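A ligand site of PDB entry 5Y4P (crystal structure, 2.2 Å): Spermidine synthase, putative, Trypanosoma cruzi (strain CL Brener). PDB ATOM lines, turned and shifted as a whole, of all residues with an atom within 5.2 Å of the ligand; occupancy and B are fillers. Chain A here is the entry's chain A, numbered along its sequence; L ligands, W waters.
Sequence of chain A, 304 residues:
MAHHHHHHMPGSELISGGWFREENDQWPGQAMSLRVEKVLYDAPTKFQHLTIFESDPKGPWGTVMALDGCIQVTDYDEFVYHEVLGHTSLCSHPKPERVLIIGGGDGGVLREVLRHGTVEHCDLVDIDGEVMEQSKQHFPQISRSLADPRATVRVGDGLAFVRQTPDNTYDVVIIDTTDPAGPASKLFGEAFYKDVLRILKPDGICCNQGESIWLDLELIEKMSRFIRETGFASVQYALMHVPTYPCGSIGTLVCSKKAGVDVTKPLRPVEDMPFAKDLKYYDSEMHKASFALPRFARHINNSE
OD1 of Asp 126 lies within hydrogen-bond range of O2 of the ligand, 2.6 Å away.
The side-chain carboxylate (OD2) of Asp 106 is in salt-bridge range of a nitrogen (N1) of the ligand (2.8 Å).
OD1 of Asp 157 lies within hydrogen-bond range of N4 of the ligand (2.8 Å).
A ring nitrogen (NE2) of His 82 sits at hydrogen-bond distance from a nitrogen (N1) of the ligand, at 2.9 Å.
An oxygen (O2) of the ligand sits at hydrogen-bond distance from the side-chain amide nitrogen of Gln 48, at 3.0 Å.
O of Asp 176 lies close to S1 of the ligand (3.7 Å).
OD2 of Asp 176 is in salt-bridge range of N1 of the ligand (3.2 Å).
A nitrogen (N5) of the ligand lies within hydrogen-bond range of the backbone NH (N) of Ile 127, at 3.1 Å.
The backbone NH of Gly 158 sits at hydrogen-bond distance from a nitrogen (N6) of the ligand.
The backbone NH (N) of Asp 128 lies close to the side-chain carboxylate (OD1) of Asp 126 (3.2 Å).
The side-chain carboxylate of Asp 126 lies within hydrogen-bond range of the backbone NH of Gly 105, 2.7 Å away.
A ring nitrogen (NE2) of His 82 lies within hydrogen-bond range of the side-chain carboxylate (OD1) of Asp 106 (3.3 Å).
OD1 of Asp 157 sits at hydrogen-bond distance from N of Leu 159 (3.1 Å).
The backbone NH (N) of Asp 176 is in hydrogen-bond range of the backbone carbonyl oxygen (O) of Ile 102, at 2.9 Å.
The backbone carbonyl oxygen of Gly 156 sits at hydrogen-bond distance from the backbone NH of Ile 127 (3.1 Å).
O of Gln 72 is in hydrogen-bond range of OH of Tyr 81 (3.5 Å).
The backbone carbonyl oxygen (O) of Met 65 is in hydrogen-bond range of the backbone NH (N) of Gln 72 (2.7 Å).
CD1 of Leu 67 touches C9 of the ligand (3.7 Å).
Gln 72 touches the ligand.
Gly 103 touches the ligand.
Gly 104 touches the ligand (N to C6, 3.9 Å).
Val 125 touches the ligand (O to C14, 3.6 Å).
CB of Asp 128 touches O2 of the ligand, at 3.6 Å.
Val 131 touches the ligand (CG1 to O3, 3.4 Å).
O of Gly 156 touches C14 of the ligand, 3.7 Å away.
Thr 177 touches the ligand (O to C5, 3.5 Å).
Hydrophobic or aromatic side chains within 4 Å of the ligand: Leu 67, His 82, Ile 127 and Val 131.
Within 4 Å of the ligand: Gln 48, Leu 67, Gln 72, His 82, Gly 103, Gly 104, Asp 106, Val 125, Asp 126, Ile 127, Asp 128, Val 131, Gly 156, Asp 157, Gly 158, Asp 176 and Thr 177.
Water W2 lies within hydrogen-bond range of OD2 of Asp 176 (2.5 Å), OD1 of Asp 106 (2.9 Å) and N1 of the ligand (3.4 Å).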
ATOM      1  N   GLN A  48      16.272  27.291 -27.034  1.00  0.00           N
ATOM      2  CA  GLN A  48      17.302  27.185 -25.971  1.00  0.00           C
ATOM      3  C   GLN A  48      18.601  27.937 -26.332  1.00  0.00           C
ATOM      4  O   GLN A  48      18.791  28.304 -27.479  1.00  0.00           O
ATOM      5  CB  GLN A  48      17.587  25.678 -25.645  1.00  0.00           C
ATOM      6  CG  GLN A  48      18.087  24.874 -26.834  1.00  0.00           C
ATOM      7  CD  GLN A  48      17.685  23.398 -26.844  1.00  0.00           C
ATOM      8  OE1 GLN A  48      17.629  22.759 -25.804  1.00  0.00           O
ATOM      9  NE2 GLN A  48      17.446  22.860 -28.043  1.00  0.00           N
ATOM     10  N   MET A  65      29.657  20.923 -27.376  1.00  0.00           N
ATOM     11  CA  MET A  65      28.324  21.525 -27.435  1.00  0.00           C
ATOM     12  C   MET A  65      27.612  21.547 -26.088  1.00  0.00           C
ATOM     13  O   MET A  65      27.491  20.501 -25.449  1.00  0.00           O
ATOM     14  CB  MET A  65      27.460  20.797 -28.477  1.00  0.00           C
ATOM     15  CG  MET A  65      26.092  21.439 -28.699  1.00  0.00           C
ATOM     16  SD  MET A  65      24.921  20.455 -29.656  1.00  0.00           S
ATOM     17  CE  MET A  65      25.775  20.310 -31.221  1.00  0.00           C
ATOM     18  N   LEU A  67      23.823  23.088 -24.245  1.00  0.00           N
ATOM     19  CA  LEU A  67      22.477  23.618 -24.401  1.00  0.00           C
ATOM     20  C   LEU A  67      22.065  24.174 -23.058  1.00  0.00           C
ATOM     21  O   LEU A  67      22.174  23.475 -22.073  1.00  0.00           O
ATOM     22  CB  LEU A  67      21.480  22.540 -24.888  1.00  0.00           C
ATOM     23  CG  LEU A  67      21.649  22.000 -26.316  1.00  0.00           C
ATOM     24  CD1 LEU A  67      20.912  20.683 -26.468  1.00  0.00           C
ATOM     25  CD2 LEU A  67      21.137  22.976 -27.363  1.00  0.00           C
ATOM     26  N   GLN A  72      26.352  18.780 -23.649  1.00  0.00           N
ATOM     27  CA  GLN A  72      25.544  17.681 -24.185  1.00  0.00           C
ATOM     28  C   GLN A  72      26.427  16.797 -25.056  1.00  0.00           C
ATOM     29  O   GLN A  72      26.191  15.610 -25.103  1.00  0.00           O
ATOM     30  CB  GLN A  72      24.365  18.195 -25.038  1.00  0.00           C
ATOM     31  CG  GLN A  72      23.447  19.198 -24.362  1.00  0.00           C
ATOM     32  CD  GLN A  72      22.414  18.550 -23.449  1.00  0.00           C
ATOM     33  OE1 GLN A  72      21.800  17.542 -23.806  1.00  0.00           O
ATOM     34  NE2 GLN A  72      22.214  19.149 -22.289  1.00  0.00           N
ATOM     35  N   VAL A  73      27.390  17.393 -25.759  1.00  0.00           N
ATOM     36  CA  VAL A  73      28.277  16.659 -26.706  1.00  0.00           C
ATOM     37  C   VAL A  73      29.724  17.162 -26.679  1.00  0.00           C
ATOM     38  O   VAL A  73      29.966  18.374 -26.779  1.00  0.00           O
ATOM     39  CB  VAL A  73      27.781  16.752 -28.188  1.00  0.00           C
ATOM     40  CG1 VAL A  73      28.795  16.134 -29.144  1.00  0.00           C
ATOM     41  CG2 VAL A  73      26.448  16.054 -28.368  1.00  0.00           C
ATOM     42  N   TYR A  81      27.641   7.534 -24.613  1.00  0.00           N
ATOM     43  CA  TYR A  81      26.180   7.688 -24.567  1.00  0.00           C
ATOM     44  C   TYR A  81      25.460   7.357 -25.873  1.00  0.00           C
ATOM     45  O   TYR A  81      24.347   6.860 -25.829  1.00  0.00           O
ATOM     46  CB  TYR A  81      25.753   9.050 -23.983  1.00  0.00           C
ATOM     47  CG  TYR A  81      26.621  10.224 -24.368  1.00  0.00           C
ATOM     48  CD1 TYR A  81      27.801  10.541 -23.635  1.00  0.00           C
ATOM     49  CD2 TYR A  81      26.262  11.035 -25.449  1.00  0.00           C
ATOM     50  CE1 TYR A  81      28.592  11.625 -23.995  1.00  0.00           C
ATOM     51  CE2 TYR A  81      27.043  12.128 -25.811  1.00  0.00           C
ATOM     52  CZ  TYR A  81      28.200  12.428 -25.091  1.00  0.00           C
ATOM     53  OH  TYR A  81      28.947  13.520 -25.491  1.00  0.00           O
ATOM     54  N   HIS A  82      26.104   7.542 -27.033  1.00  0.00           N
ATOM     55  CA  HIS A  82      25.505   7.126 -28.316  1.00  0.00           C
ATOM     56  C   HIS A  82      25.524   5.623 -28.588  1.00  0.00           C
ATOM     57  O   HIS A  82      24.549   5.076 -29.132  1.00  0.00           O
ATOM     58  CB  HIS A  82      26.084   7.914 -29.470  1.00  0.00           C
ATOM     59  CG  HIS A  82      25.884   9.397 -29.344  1.00  0.00           C
ATOM     60  ND1 HIS A  82      26.847  10.303 -29.742  1.00  0.00           N
ATOM     61  CD2 HIS A  82      24.869  10.121 -28.829  1.00  0.00           C
ATOM     62  CE1 HIS A  82      26.413  11.529 -29.507  1.00  0.00           C
ATOM     63  NE2 HIS A  82      25.218  11.446 -28.951  1.00  0.00           N
ATOM     64  N   ILE A 102      13.648  10.589 -30.491  1.00  0.00           N
ATOM     65  CA  ILE A 102      13.169  11.873 -30.049  1.00  0.00           C
ATOM     66  C   ILE A 102      14.349  12.642 -29.504  1.00  0.00           C
ATOM     67  O   ILE A 102      15.030  12.177 -28.579  1.00  0.00           O
ATOM     68  CB  ILE A 102      11.999  11.700 -29.038  1.00  0.00           C
ATOM     69  CG1 ILE A 102      10.717  11.369 -29.823  1.00  0.00           C
ATOM     70  CG2 ILE A 102      11.795  12.967 -28.205  1.00  0.00           C
ATOM     71  CD1 ILE A 102       9.721  10.529 -29.054  1.00  0.00           C
ATOM     72  N   GLY A 103      14.582  13.832 -30.069  1.00  0.00           N
ATOM     73  CA  GLY A 103      15.775  14.614 -29.797  1.00  0.00           C
ATOM     74  C   GLY A 103      16.861  14.147 -30.752  1.00  0.00           C
ATOM     75  O   GLY A 103      16.586  13.901 -31.927  1.00  0.00           O
ATOM     76  N   GLY A 104      18.088  14.014 -30.266  1.00  0.00           N
ATOM     77  CA  GLY A 104      19.153  13.346 -31.029  1.00  0.00           C
ATOM     78  C   GLY A 104      19.599  14.081 -32.270  1.00  0.00           C
ATOM     79  O   GLY A 104      20.120  13.472 -33.233  1.00  0.00           O
ATOM     80  N   GLY A 105      19.419  15.390 -32.245  1.00  0.00           N
ATOM     81  CA  GLY A 105      19.602  16.252 -33.404  1.00  0.00           C
ATOM     82  C   GLY A 105      21.023  16.359 -33.838  1.00  0.00           C
ATOM     83  O   GLY A 105      21.290  16.782 -34.956  1.00  0.00           O
ATOM     84  N   ASP A 106      21.944  15.991 -32.944  1.00  0.00           N
ATOM     85  CA  ASP A 106      23.367  15.897 -33.270  1.00  0.00           C
ATOM     86  C   ASP A 106      23.679  14.727 -34.224  1.00  0.00           C
ATOM     87  O   ASP A 106      24.725  14.717 -34.878  1.00  0.00           O
ATOM     88  CB  ASP A 106      24.196  15.754 -31.989  1.00  0.00           C
ATOM     89  CG  ASP A 106      23.737  14.607 -31.137  1.00  0.00           C
ATOM     90  OD1 ASP A 106      24.195  13.442 -31.354  1.00  0.00           O
ATOM     91  OD2 ASP A 106      22.896  14.887 -30.252  1.00  0.00           O
ATOM     92  N   VAL A 125      13.083  13.126 -34.637  1.00  0.00           N
ATOM     93  CA  VAL A 125      12.388  14.396 -34.386  1.00  0.00           C
ATOM     94  C   VAL A 125      13.100  15.188 -33.288  1.00  0.00           C
ATOM     95  O   VAL A 125      13.144  14.761 -32.136  1.00  0.00           O
ATOM     96  CB  VAL A 125      10.898  14.180 -33.966  1.00  0.00           C
ATOM     97  CG1 VAL A 125      10.121  15.474 -34.119  1.00  0.00           C
ATOM     98  CG2 VAL A 125      10.238  13.071 -34.776  1.00  0.00           C
ATOM     99  N   ASP A 126      13.613  16.348 -33.653  1.00  0.00           N
ATOM    100  CA  ASP A 126      14.277  17.242 -32.704  1.00  0.00           C
ATOM    101  C   ASP A 126      13.603  18.623 -32.816  1.00  0.00           C
ATOM    102  O   ASP A 126      13.496  19.159 -33.916  1.00  0.00           O
ATOM    103  CB  ASP A 126      15.796  17.330 -32.999  1.00  0.00           C
ATOM    104  CG  ASP A 126      16.623  17.902 -31.833  1.00  0.00           C
ATOM    105  OD1 ASP A 126      16.372  19.056 -31.389  1.00  0.00           O
ATOM    106  OD2 ASP A 126      17.528  17.167 -31.354  1.00  0.00           O
ATOM    107  N   ILE A 127      13.168  19.194 -31.686  1.00  0.00           N
ATOM    108  CA  ILE A 127      12.450  20.479 -31.647  1.00  0.00           C
ATOM    109  C   ILE A 127      13.198  21.638 -32.283  1.00  0.00           C
ATOM    110  O   ILE A 127      12.592  22.568 -32.791  1.00  0.00           O
ATOM    111  CB  ILE A 127      11.936  20.835 -30.213  1.00  0.00           C
ATOM    112  CG1 ILE A 127      10.739  21.812 -30.292  1.00  0.00           C
ATOM    113  CG2 ILE A 127      13.072  21.311 -29.311  1.00  0.00           C
ATOM    114  CD1 ILE A 127       9.878  21.931 -29.041  1.00  0.00           C
ATOM    115  N   ASP A 128      14.520  21.531 -32.282  1.00  0.00           N
ATOM    116  CA  ASP A 128      15.407  22.630 -32.603  1.00  0.00           C
ATOM    117  C   ASP A 128      16.232  22.317 -33.838  1.00  0.00           C
ATOM    118  O   ASP A 128      17.235  21.601 -33.773  1.00  0.00           O
ATOM    119  CB  ASP A 128      16.290  22.894 -31.376  1.00  0.00           C
ATOM    120  CG  ASP A 128      17.081  24.201 -31.456  1.00  0.00           C
ATOM    121  OD1 ASP A 128      17.183  24.865 -32.510  1.00  0.00           O
ATOM    122  OD2 ASP A 128      17.628  24.587 -30.398  1.00  0.00           O
ATOM    123  N   VAL A 131      20.223  23.144 -33.693  1.00  0.00           N
ATOM    124  CA  VAL A 131      21.063  22.024 -33.209  1.00  0.00           C
ATOM    125  C   VAL A 131      21.582  21.179 -34.388  1.00  0.00           C
ATOM    126  O   VAL A 131      22.799  21.062 -34.572  1.00  0.00           O
ATOM    127  CB  VAL A 131      20.337  21.144 -32.154  1.00  0.00           C
ATOM    128  CG1 VAL A 131      21.183  19.935 -31.747  1.00  0.00           C
ATOM    129  CG2 VAL A 131      19.967  21.950 -30.923  1.00  0.00           C
ATOM    130  N   GLY A 156      10.539  19.569 -34.843  1.00  0.00           N
ATOM    131  CA  GLY A 156       9.237  19.607 -34.176  1.00  0.00           C
ATOM    132  C   GLY A 156       9.265  18.978 -32.802  1.00  0.00           C
ATOM    133  O   GLY A 156      10.233  18.328 -32.413  1.00  0.00           O
ATOM    134  N   ASP A 157       8.178  19.158 -32.060  1.00  0.00           N
ATOM    135  CA  ASP A 157       8.063  18.640 -30.718  1.00  0.00           C
ATOM    136  C   ASP A 157       7.675  17.147 -30.737  1.00  0.00           C
ATOM    137  O   ASP A 157       6.672  16.756 -31.356  1.00  0.00           O
ATOM    138  CB  ASP A 157       7.036  19.482 -29.919  1.00  0.00           C
ATOM    139  CG  ASP A 157       6.991  19.141 -28.420  1.00  0.00           C
ATOM    140  OD1 ASP A 157       7.765  18.297 -27.921  1.00  0.00           O
ATOM    141  OD2 ASP A 157       6.150  19.735 -27.729  1.00  0.00           O
ATOM    142  N   GLY A 158       8.465  16.333 -30.035  1.00  0.00           N
ATOM    143  CA  GLY A 158       8.212  14.907 -29.886  1.00  0.00           C
ATOM    144  C   GLY A 158       6.906  14.591 -29.180  1.00  0.00           C
ATOM    145  O   GLY A 158       6.296  13.570 -29.460  1.00  0.00           O
ATOM    146  N   LEU A 159       6.497  15.478 -28.282  1.00  0.00           N
ATOM    147  CA  LEU A 159       5.208  15.347 -27.582  1.00  0.00           C
ATOM    148  C   LEU A 159       4.079  15.418 -28.595  1.00  0.00           C
ATOM    149  O   LEU A 159       3.196  14.565 -28.598  1.00  0.00           O
ATOM    150  CB  LEU A 159       5.044  16.443 -26.522  1.00  0.00           C
ATOM    151  CG  LEU A 159       3.693  16.602 -25.825  1.00  0.00           C
ATOM    152  CD1 LEU A 159       3.535  15.671 -24.614  1.00  0.00           C
ATOM    153  CD2 LEU A 159       3.534  18.067 -25.433  1.00  0.00           C
ATOM    154  N   ASP A 176      16.402  10.741 -26.478  1.00  0.00           N
ATOM    155  CA  ASP A 176      17.730  11.324 -26.322  1.00  0.00           C
ATOM    156  C   ASP A 176      17.652  12.840 -26.097  1.00  0.00           C
ATOM    157  O   ASP A 176      18.115  13.617 -26.932  1.00  0.00           O
ATOM    158  CB  ASP A 176      18.542  11.013 -27.598  1.00  0.00           C
ATOM    159  CG  ASP A 176      19.997  11.507 -27.553  1.00  0.00           C
ATOM    160  OD1 ASP A 176      20.561  11.716 -26.473  1.00  0.00           O
ATOM    161  OD2 ASP A 176      20.585  11.685 -28.643  1.00  0.00           O
ATOM    162  N   THR A 177      17.083  13.274 -24.981  1.00  0.00           N
ATOM    163  CA  THR A 177      16.923  14.701 -24.697  1.00  0.00           C
ATOM    164  C   THR A 177      17.845  15.149 -23.561  1.00  0.00           C
ATOM    165  O   THR A 177      18.558  16.154 -23.694  1.00  0.00           O
ATOM    166  CB  THR A 177      15.466  15.063 -24.358  1.00  0.00           C
ATOM    167  OG1 THR A 177      15.070  14.329 -23.192  1.00  0.00           O
ATOM    168  CG2 THR A 177      14.550  14.714 -25.503  1.00  0.00           C
HETATM  169  C1  LIG L   1      23.330  13.683 -26.523  1.00  0.00           C
HETATM  170  N1  LIG L   1      23.237  13.360 -27.966  1.00  0.00           N
HETATM  171  C2  LIG L   1      22.031  14.352 -26.135  1.00  0.00           C
HETATM  172  C3  LIG L   1      21.944  15.782 -26.576  1.00  0.00           C
HETATM  173  S1  LIG L   1      20.803  15.963 -27.990  1.00  0.00           S
HETATM  174  C4  LIG L   1      21.676  17.467 -28.506  1.00  0.00           C
HETATM  175  C5  LIG L   1      19.422  16.728 -27.039  1.00  0.00           C
HETATM  176  C6  LIG L   1      18.284  17.195 -27.944  1.00  0.00           C
HETATM  177  O1  LIG L   1      16.964  17.024 -27.409  1.00  0.00           O
HETATM  178  C7  LIG L   1      16.166  18.021 -28.097  1.00  0.00           C
HETATM  179  C8  LIG L   1      17.015  19.261 -28.005  1.00  0.00           C
HETATM  180  O2  LIG L   1      16.623  20.153 -29.012  1.00  0.00           O
HETATM  181  C9  LIG L   1      18.395  18.679 -28.203  1.00  0.00           C
HETATM  182  O3  LIG L   1      18.866  18.733 -29.533  1.00  0.00           O
HETATM  183  N2  LIG L   1      14.837  18.165 -27.502  1.00  0.00           N
HETATM  184  C10 LIG L   1      14.517  18.698 -26.276  1.00  0.00           C
HETATM  185  N3  LIG L   1      13.212  18.684 -26.049  1.00  0.00           N
HETATM  186  C11 LIG L   1      12.663  18.115 -27.180  1.00  0.00           C
HETATM  187  C12 LIG L   1      11.349  17.851 -27.529  1.00  0.00           C
HETATM  188  N4  LIG L   1      10.273  18.132 -26.686  1.00  0.00           N
HETATM  189  C13 LIG L   1      13.660  17.792 -28.081  1.00  0.00           C
HETATM  190  N5  LIG L   1      13.492  17.246 -29.295  1.00  0.00           N
HETATM  191  C14 LIG L   1      12.191  17.018 -29.511  1.00  0.00           C
HETATM  192  N6  LIG L   1      11.135  17.278 -28.729  1.00  0.00           N
HETATM  193  O   HOH W   1      20.442  12.589 -23.910  1.00  0.00           O
HETATM  194  O   HOH W   2      21.961  11.702 -30.700  1.00  0.00           O
